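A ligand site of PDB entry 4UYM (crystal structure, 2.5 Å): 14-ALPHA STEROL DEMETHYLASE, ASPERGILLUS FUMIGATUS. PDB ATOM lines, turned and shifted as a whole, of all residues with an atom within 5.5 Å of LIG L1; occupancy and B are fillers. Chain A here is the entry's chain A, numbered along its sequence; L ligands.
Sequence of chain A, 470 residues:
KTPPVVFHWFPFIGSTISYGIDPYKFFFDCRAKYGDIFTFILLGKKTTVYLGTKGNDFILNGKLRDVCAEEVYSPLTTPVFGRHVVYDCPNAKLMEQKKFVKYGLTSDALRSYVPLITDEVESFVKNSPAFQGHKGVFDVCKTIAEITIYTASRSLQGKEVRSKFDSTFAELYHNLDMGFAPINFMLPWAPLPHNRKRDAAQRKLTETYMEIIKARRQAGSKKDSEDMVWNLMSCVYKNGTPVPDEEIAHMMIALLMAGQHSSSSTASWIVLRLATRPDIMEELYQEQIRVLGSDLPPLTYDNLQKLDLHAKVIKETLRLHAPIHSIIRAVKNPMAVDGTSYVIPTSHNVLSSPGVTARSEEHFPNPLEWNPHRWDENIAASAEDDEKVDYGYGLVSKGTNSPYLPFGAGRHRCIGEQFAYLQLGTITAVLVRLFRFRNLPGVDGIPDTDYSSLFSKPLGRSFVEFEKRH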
ATOM      1  N   TYR A  73      -4.879   0.500  -9.651  1.00  0.00           N
ATOM      2  CA  TYR A  73      -5.530   0.877 -10.900  1.00  0.00           C
ATOM      3  C   TYR A  73      -4.804   0.357 -12.142  1.00  0.00           C
ATOM      4  O   TYR A  73      -5.399   0.258 -13.215  1.00  0.00           O
ATOM      5  CB  TYR A  73      -5.678   2.393 -10.979  1.00  0.00           C
ATOM      6  CG  TYR A  73      -6.753   2.932 -10.058  1.00  0.00           C
ATOM      7  CD1 TYR A  73      -8.076   2.542 -10.203  1.00  0.00           C
ATOM      8  CD2 TYR A  73      -6.427   3.782  -8.997  1.00  0.00           C
ATOM      9  CE1 TYR A  73      -9.054   2.998  -9.332  1.00  0.00           C
ATOM     10  CE2 TYR A  73      -7.403   4.233  -8.133  1.00  0.00           C
ATOM     11  CZ  TYR A  73      -8.708   3.844  -8.301  1.00  0.00           C
ATOM     12  OH  TYR A  73      -9.687   4.303  -7.443  1.00  0.00           O
ATOM     13  N   THR A  77      -6.439  -0.076 -15.859  1.00  0.00           N
ATOM     14  CA  THR A  77      -6.190   1.077 -16.727  1.00  0.00           C
ATOM     15  C   THR A  77      -5.149   0.753 -17.796  1.00  0.00           C
ATOM     16  O   THR A  77      -5.262   1.210 -18.935  1.00  0.00           O
ATOM     17  CB  THR A  77      -5.710   2.292 -15.926  1.00  0.00           C
ATOM     18  OG1 THR A  77      -4.517   1.966 -15.204  1.00  0.00           O
ATOM     19  CG2 THR A  77      -6.780   2.757 -14.951  1.00  0.00           C
ATOM     20  N   PHE A  81      -5.001   2.278 -21.579  1.00  0.00           N
ATOM     21  CA  PHE A  81      -4.189   3.425 -21.987  1.00  0.00           C
ATOM     22  C   PHE A  81      -2.975   2.968 -22.781  1.00  0.00           C
ATOM     23  O   PHE A  81      -2.654   3.529 -23.834  1.00  0.00           O
ATOM     24  CB  PHE A  81      -3.723   4.224 -20.766  1.00  0.00           C
ATOM     25  CG  PHE A  81      -4.848   4.712 -19.904  1.00  0.00           C
ATOM     26  CD1 PHE A  81      -6.088   4.982 -20.458  1.00  0.00           C
ATOM     27  CD2 PHE A  81      -4.664   4.900 -18.543  1.00  0.00           C
ATOM     28  CE1 PHE A  81      -7.137   5.415 -19.668  1.00  0.00           C
ATOM     29  CE2 PHE A  81      -5.705   5.343 -17.746  1.00  0.00           C
ATOM     30  CZ  PHE A  81      -6.943   5.607 -18.307  1.00  0.00           C
ATOM     31  N   VAL A  86       1.104   6.887 -17.043  1.00  0.00           N
ATOM     32  CA  VAL A  86       0.157   6.844 -15.983  1.00  0.00           C
ATOM     33  C   VAL A  86       0.646   5.803 -15.007  1.00  0.00           C
ATOM     34  O   VAL A  86       1.644   6.014 -14.366  1.00  0.00           O
ATOM     35  CB  VAL A  86      -1.236   6.574 -16.499  1.00  0.00           C
ATOM     36  CG1 VAL A  86      -2.257   6.837 -15.434  1.00  0.00           C
ATOM     37  CG2 VAL A  86      -1.500   7.509 -17.647  1.00  0.00           C
ATOM     38  N   TYR A  87      -0.077   4.730 -14.834  1.00  0.00           N
ATOM     39  CA  TYR A  87       0.241   3.775 -13.787  1.00  0.00           C
ATOM     40  C   TYR A  87       1.167   2.644 -14.148  1.00  0.00           C
ATOM     41  O   TYR A  87       1.370   1.742 -13.369  1.00  0.00           O
ATOM     42  CB  TYR A  87      -1.029   3.249 -13.181  1.00  0.00           C
ATOM     43  CG  TYR A  87      -1.874   4.350 -12.660  1.00  0.00           C
ATOM     44  CD1 TYR A  87      -1.342   5.303 -11.848  1.00  0.00           C
ATOM     45  CD2 TYR A  87      -3.198   4.429 -12.980  1.00  0.00           C
ATOM     46  CE1 TYR A  87      -2.121   6.325 -11.359  1.00  0.00           C
ATOM     47  CE2 TYR A  87      -3.975   5.445 -12.498  1.00  0.00           C
ATOM     48  CZ  TYR A  87      -3.421   6.390 -11.689  1.00  0.00           C
ATOM     49  OH  TYR A  87      -4.184   7.396 -11.210  1.00  0.00           O
ATOM     50  N   PHE A 180     -13.397  -0.890 -19.654  1.00  0.00           N
ATOM     51  CA  PHE A 180     -13.880  -0.399 -18.374  1.00  0.00           C
ATOM     52  C   PHE A 180     -15.145  -1.141 -17.948  1.00  0.00           C
ATOM     53  O   PHE A 180     -16.014  -0.597 -17.269  1.00  0.00           O
ATOM     54  CB  PHE A 180     -14.170   1.102 -18.442  1.00  0.00           C
ATOM     55  CG  PHE A 180     -12.943   1.956 -18.334  1.00  0.00           C
ATOM     56  CD1 PHE A 180     -12.013   1.715 -17.346  1.00  0.00           C
ATOM     57  CD2 PHE A 180     -12.701   2.958 -19.257  1.00  0.00           C
ATOM     58  CE1 PHE A 180     -10.863   2.480 -17.249  1.00  0.00           C
ATOM     59  CE2 PHE A 180     -11.554   3.730 -19.167  1.00  0.00           C
ATOM     60  CZ  PHE A 180     -10.636   3.492 -18.170  1.00  0.00           C
ATOM     61  N   ALA A 254      -4.812   8.106 -22.821  1.00  0.00           N
ATOM     62  CA  ALA A 254      -5.189   8.281 -21.422  1.00  0.00           C
ATOM     63  C   ALA A 254      -6.012   9.554 -21.231  1.00  0.00           C
ATOM     64  O   ALA A 254      -7.045   9.549 -20.572  1.00  0.00           O
ATOM     65  CB  ALA A 254      -3.954   8.316 -20.541  1.00  0.00           C
ATOM     66  N   ALA A 258      -9.914   9.662 -20.150  1.00  0.00           N
ATOM     67  CA  ALA A 258     -10.139  10.394 -18.899  1.00  0.00           C
ATOM     68  C   ALA A 258     -11.089  11.571 -19.096  1.00  0.00           C
ATOM     69  O   ALA A 258     -12.089  11.698 -18.402  1.00  0.00           O
ATOM     70  CB  ALA A 258      -8.816  10.863 -18.314  1.00  0.00           C
ATOM     71  N   GLY A 259     -10.727  12.454 -20.025  1.00  0.00           N
ATOM     72  CA  GLY A 259     -11.519  13.652 -20.285  1.00  0.00           C
ATOM     73  C   GLY A 259     -12.938  13.314 -20.707  1.00  0.00           C
ATOM     74  O   GLY A 259     -13.909  13.857 -20.169  1.00  0.00           O
ATOM     75  N   SER A 262     -15.227  11.758 -17.838  1.00  0.00           N
ATOM     76  CA  SER A 262     -15.478  12.765 -16.814  1.00  0.00           C
ATOM     77  C   SER A 262     -16.363  13.871 -17.371  1.00  0.00           C
ATOM     78  O   SER A 262     -17.348  14.274 -16.735  1.00  0.00           O
ATOM     79  CB  SER A 262     -14.158  13.360 -16.319  1.00  0.00           C
ATOM     80  OG  SER A 262     -13.197  13.395 -17.347  1.00  0.00           O
ATOM     81  N   ILE A 324     -16.100  10.547 -10.196  1.00  0.00           N
ATOM     82  CA  ILE A 324     -15.300   9.779  -9.250  1.00  0.00           C
ATOM     83  C   ILE A 324     -15.896   9.848  -7.850  1.00  0.00           C
ATOM     84  O   ILE A 324     -15.973  10.926  -7.256  1.00  0.00           O
ATOM     85  CB  ILE A 324     -13.837  10.277  -9.183  1.00  0.00           C
ATOM     86  CG1 ILE A 324     -13.090   9.914 -10.472  1.00  0.00           C
ATOM     87  CG2 ILE A 324     -13.126   9.667  -7.993  1.00  0.00           C
ATOM     88  CD1 ILE A 324     -13.418  10.811 -11.640  1.00  0.00           C
ATOM     89  N   HIS A 325     -16.324   8.704  -7.329  1.00  0.00           N
ATOM     90  CA  HIS A 325     -16.898   8.662  -5.982  1.00  0.00           C
ATOM     91  C   HIS A 325     -15.918   8.101  -4.954  1.00  0.00           C
ATOM     92  O   HIS A 325     -15.933   8.485  -3.792  1.00  0.00           O
ATOM     93  CB  HIS A 325     -18.177   7.826  -5.975  1.00  0.00           C
ATOM     94  CG  HIS A 325     -18.045   6.494  -6.650  1.00  0.00           C
ATOM     95  ND1 HIS A 325     -17.292   5.465  -6.121  1.00  0.00           N
ATOM     96  CD2 HIS A 325     -18.606   6.010  -7.777  1.00  0.00           C
ATOM     97  CE1 HIS A 325     -17.371   4.415  -6.911  1.00  0.00           C
ATOM     98  NE2 HIS A 325     -18.164   4.719  -7.933  1.00  0.00           N
ATOM     99  N   SER A 326     -15.072   7.176  -5.402  1.00  0.00           N
ATOM    100  CA  SER A 326     -14.170   6.470  -4.508  1.00  0.00           C
ATOM    101  C   SER A 326     -12.728   6.610  -4.995  1.00  0.00           C
ATOM    102  O   SER A 326     -12.413   6.277  -6.130  1.00  0.00           O
ATOM    103  CB  SER A 326     -14.537   4.994  -4.409  1.00  0.00           C
ATOM    104  OG  SER A 326     -15.904   4.825  -4.062  1.00  0.00           O
ATOM    105  N   ILE A 327     -11.856   7.095  -4.113  1.00  0.00           N
ATOM    106  CA  ILE A 327     -10.431   7.091  -4.388  1.00  0.00           C
ATOM    107  C   ILE A 327      -9.734   6.075  -3.493  1.00  0.00           C
ATOM    108  O   ILE A 327      -9.943   6.053  -2.272  1.00  0.00           O
ATOM    109  CB  ILE A 327      -9.797   8.478  -4.167  1.00  0.00           C
ATOM    110  CG1 ILE A 327     -10.595   9.543  -4.916  1.00  0.00           C
ATOM    111  CG2 ILE A 327      -8.351   8.474  -4.637  1.00  0.00           C
ATOM    112  CD1 ILE A 327      -9.966  10.918  -4.861  1.00  0.00           C
ATOM    113  N   ILE A 328      -8.905   5.239  -4.107  1.00  0.00           N
ATOM    114  CA  ILE A 328      -8.398   4.050  -3.432  1.00  0.00           C
ATOM    115  C   ILE A 328      -6.879   3.948  -3.521  1.00  0.00           C
ATOM    116  O   ILE A 328      -6.283   4.203  -4.570  1.00  0.00           O
ATOM    117  CB  ILE A 328      -9.010   2.765  -4.007  1.00  0.00           C
ATOM    118  CG1 ILE A 328     -10.532   2.792  -3.827  1.00  0.00           C
ATOM    119  CG2 ILE A 328      -8.428   1.544  -3.307  1.00  0.00           C
ATOM    120  CD1 ILE A 328     -11.239   1.649  -4.532  1.00  0.00           C
ATOM    121  N   CYS A 414      -5.974  16.384  -9.838  1.00  0.00           N
ATOM    122  CA  CYS A 414      -6.242  16.517 -11.256  1.00  0.00           C
ATOM    123  C   CYS A 414      -5.395  17.617 -11.874  1.00  0.00           C
ATOM    124  O   CYS A 414      -5.279  18.709 -11.319  1.00  0.00           O
ATOM    125  CB  CYS A 414      -7.728  16.824 -11.494  1.00  0.00           C
ATOM    126  SG  CYS A 414      -8.323  16.390 -13.134  1.00  0.00           S
ATOM    127  N   LEU A 454     -16.728   2.154 -13.698  1.00  0.00           N
ATOM    128  CA  LEU A 454     -15.663   2.889 -13.024  1.00  0.00           C
ATOM    129  C   LEU A 454     -16.061   4.351 -12.822  1.00  0.00           C
ATOM    130  O   LEU A 454     -15.928   4.887 -11.718  1.00  0.00           O
ATOM    131  CB  LEU A 454     -14.368   2.804 -13.835  1.00  0.00           C
ATOM    132  CG  LEU A 454     -13.168   3.560 -13.264  1.00  0.00           C
ATOM    133  CD1 LEU A 454     -12.735   2.990 -11.927  1.00  0.00           C
ATOM    134  CD2 LEU A 454     -12.008   3.537 -14.254  1.00  0.00           C
ATOM    135  N   PHE A 455     -16.468   5.018 -13.877  1.00  0.00           N
ATOM    136  CA  PHE A 455     -17.063   6.322 -13.769  1.00  0.00           C
ATOM    137  C   PHE A 455     -18.541   6.121 -13.530  1.00  0.00           C
ATOM    138  O   PHE A 455     -19.045   5.096 -13.888  1.00  0.00           O
ATOM    139  CB  PHE A 455     -16.806   7.119 -15.014  1.00  0.00           C
ATOM    140  CG  PHE A 455     -15.360   7.381 -15.278  1.00  0.00           C
ATOM    141  CD1 PHE A 455     -14.562   6.397 -15.779  1.00  0.00           C
ATOM    142  CD2 PHE A 455     -14.825   8.617 -15.052  1.00  0.00           C
ATOM    143  CE1 PHE A 455     -13.236   6.643 -16.026  1.00  0.00           C
ATOM    144  CE2 PHE A 455     -13.501   8.870 -15.305  1.00  0.00           C
ATOM    145  CZ  PHE A 455     -12.710   7.876 -15.800  1.00  0.00           C
HETATM  146  F1  LIG L   1      -9.446   7.071 -15.127  1.00  0.00           F
HETATM  147  F2  LIG L   1     -12.445   6.272 -12.411  1.00  0.00           F
HETATM  148  F3  LIG L   1      -5.383   9.146 -16.402  1.00  0.00           F
HETATM  149  O1  LIG L   1      -8.954   8.922 -11.241  1.00  0.00           O
HETATM  150  N1  LIG L   1     -10.234  10.288 -13.466  1.00  0.00           N
HETATM  151  N2  LIG L   1      -9.954   6.698  -9.760  1.00  0.00           N
HETATM  152  N3  LIG L   1     -11.021  10.799 -14.511  1.00  0.00           N
HETATM  153  N4  LIG L   1      -9.395  12.189 -13.999  1.00  0.00           N
HETATM  154  N5  LIG L   1     -12.066   6.298  -8.841  1.00  0.00           N
HETATM  155  C1  LIG L   1      -9.332   8.276 -12.457  1.00  0.00           C
HETATM  156  C2  LIG L   1      -9.572   6.790 -12.192  1.00  0.00           C
HETATM  157  C3  LIG L   1     -10.582   8.941 -13.022  1.00  0.00           C
HETATM  158  C4  LIG L   1      -8.247   8.452 -13.478  1.00  0.00           C
HETATM  159  C5  LIG L   1      -8.260   6.035 -11.975  1.00  0.00           C
HETATM  160  C6  LIG L   1     -10.443   6.630 -11.011  1.00  0.00           C
HETATM  161  C7  LIG L   1      -8.398   7.861 -14.831  1.00  0.00           C
HETATM  162  C8  LIG L   1      -7.167   9.298 -13.228  1.00  0.00           C
HETATM  163  C9  LIG L   1     -11.899   6.354 -11.185  1.00  0.00           C
HETATM  164  C10 LIG L   1      -7.415   8.107 -15.782  1.00  0.00           C
HETATM  165  C11 LIG L   1      -6.215   9.503 -14.218  1.00  0.00           C
HETATM  166  C12 LIG L   1      -9.220  11.112 -13.212  1.00  0.00           C
HETATM  167  C13 LIG L   1      -6.332   8.922 -15.472  1.00  0.00           C
HETATM  168  C14 LIG L   1     -12.657   6.197 -10.036  1.00  0.00           C
HETATM  169  C15 LIG L   1     -10.760   6.542  -8.706  1.00  0.00           C
HETATM  170  C16 LIG L   1     -10.482  12.004 -14.785  1.00  0.00           C
HETATM  171  C1  LG2 L   2      -6.765  13.025 -11.257  1.00  0.00           C
HETATM  172  C2  LG2 L   2     -11.387  14.101 -11.189  1.00  0.00           C
HETATM  173  C3  LG2 L   2     -11.036  15.726 -15.666  1.00  0.00           C
HETATM  174  C4  LG2 L   2      -6.684  13.908 -15.920  1.00  0.00           C
HETATM  175  C5  LG2 L   2      -8.048  13.224 -10.898  1.00  0.00           C
HETATM  176  C6  LG2 L   2      -8.516  12.935  -9.630  1.00  0.00           C
HETATM  177  C7  LG2 L   2      -9.814  13.226  -9.587  1.00  0.00           C
HETATM  178  C8  LG2 L   2     -10.153  13.713 -10.837  1.00  0.00           C
HETATM  179  C9  LG2 L   2     -10.703  13.055  -8.413  1.00  0.00           C
HETATM  180  C10 LG2 L   2      -7.702  12.352  -8.503  1.00  0.00           C
HETATM  181  C11 LG2 L   2      -7.913  10.823  -8.340  1.00  0.00           C
HETATM  182  C12 LG2 L   2      -6.788  10.042  -7.664  1.00  0.00           C
HETATM  183  O1  LG2 L   2      -6.686   8.846  -7.896  1.00  0.00           O
HETATM  184  O2  LG2 L   2      -6.020  10.622  -6.781  1.00  0.00           O
HETATM  185  C13 LG2 L   2     -11.630  14.652 -12.418  1.00  0.00           C
HETATM  186  C14 LG2 L   2     -12.881  15.169 -12.716  1.00  0.00           C
HETATM  187  C15 LG2 L   2     -12.804  15.634 -13.966  1.00  0.00           C
HETATM  188  C16 LG2 L   2     -11.454  15.373 -14.418  1.00  0.00           C
HETATM  189  C17 LG2 L   2     -14.052  15.182 -11.783  1.00  0.00           C
HETATM  190  C18 LG2 L   2     -13.819  16.278 -14.786  1.00  0.00           C
HETATM  191  C19 LG2 L   2     -14.814  16.927 -14.252  1.00  0.00           C
HETATM  192  C20 LG2 L   2      -9.815  15.368 -16.133  1.00  0.00           C
HETATM  193  C21 LG2 L   2      -9.349  15.637 -17.375  1.00  0.00           C
HETATM  194  C22 LG2 L   2      -8.094  15.108 -17.453  1.00  0.00           C
HETATM  195  C23 LG2 L   2      -7.824  14.536 -16.228  1.00  0.00           C
HETATM  196  C24 LG2 L   2     -10.101  16.369 -18.424  1.00  0.00           C
HETATM  197  C25 LG2 L   2      -7.194  15.150 -18.595  1.00  0.00           C
HETATM  198  C26 LG2 L   2      -7.304  16.105 -19.483  1.00  0.00           C
HETATM  199  C27 LG2 L   2      -6.408  13.560 -14.632  1.00  0.00           C
HETATM  200  C28 LG2 L   2      -5.102  13.077 -14.299  1.00  0.00           C
HETATM  201  C29 LG2 L   2      -5.108  12.823 -13.014  1.00  0.00           C
HETATM  202  C30 LG2 L   2      -6.428  13.189 -12.558  1.00  0.00           C
HETATM  203  C31 LG2 L   2      -3.935  12.880 -15.212  1.00  0.00           C
HETATM  204  C32 LG2 L   2      -3.947  12.311 -12.227  1.00  0.00           C
HETATM  205  C33 LG2 L   2      -4.275  11.150 -11.316  1.00  0.00           C
HETATM  206  C34 LG2 L   2      -3.013  10.662 -10.665  1.00  0.00           C
HETATM  207  O3  LG2 L   2      -2.991   9.561 -10.110  1.00  0.00           O
HETATM  208  O4  LG2 L   2      -1.981  11.316 -10.672  1.00  0.00           O
HETATM  209  N1  LG2 L   2      -9.077  13.657 -11.644  1.00  0.00           N
HETATM  210  N2  LG2 L   2     -10.825  14.786 -13.432  1.00  0.00           N
HETATM  211  N3  LG2 L   2      -8.900  14.686 -15.452  1.00  0.00           N
HETATM  212  N4  LG2 L   2      -7.171  13.602 -13.563  1.00  0.00           N
HETATM  213 FE1  LG2 L   2      -8.881  14.173 -13.494  1.00  0.00          FE
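The side-chain hydroxyl (OH) of Tyr 87 lies within hydrogen-bond range of an oxygen (O3) of LG2 L2, 2.7 Å away.
SG of Cys 414 binds FE1 of LG2 L2, 2.3 Å away.
OH of Tyr 73 sits close to N2 of LIG L1, 3.3 Å away.
A nitrogen (N5) of LIG L1 lies close to the backbone carbonyl oxygen (O) of Ser 326 (2.7 Å).
An iron atom (FE1) of LG2 L2 is bound by a nitrogen (N4) of LIG L1.
A ring nitrogen (ND1) of His 325 sits at hydrogen-bond distance from the side-chain hydroxyl of Ser 326 (2.6 Å).
O of Gly 259 is in hydrogen-bond range of OG of Ser 262, at 2.9 Å.
The backbone carbonyl oxygen (O) of Tyr 73 lies within hydrogen-bond range of the side-chain hydroxyl (OG1) of Thr 77.
Phe 81 touches LIG L1 (CZ to C10, 3.6 Å).
O of Ala 258 touches C16 of LIG L1, 3.97 Å away.
OG of Ser 262 touches C16 of LIG L1 (3.98 Å).
Ile 324 touches LIG L1.
Leu 454 touches LIG L1 (CG to F2, 2.9 Å).
CE2 of Phe 455 touches N3 of LIG L1 (3.2 Å).
Hydrophobic or aromatic side chains that line LIG L1: Tyr 73, Phe 81, Ala 258, Ile 324, Leu 454 and Phe 455.
Within 4 Å of LIG L1: Tyr 73, Phe 81, Ala 258, Ser 262, Ile 324, Ser 326, Leu 454 and Phe 455.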
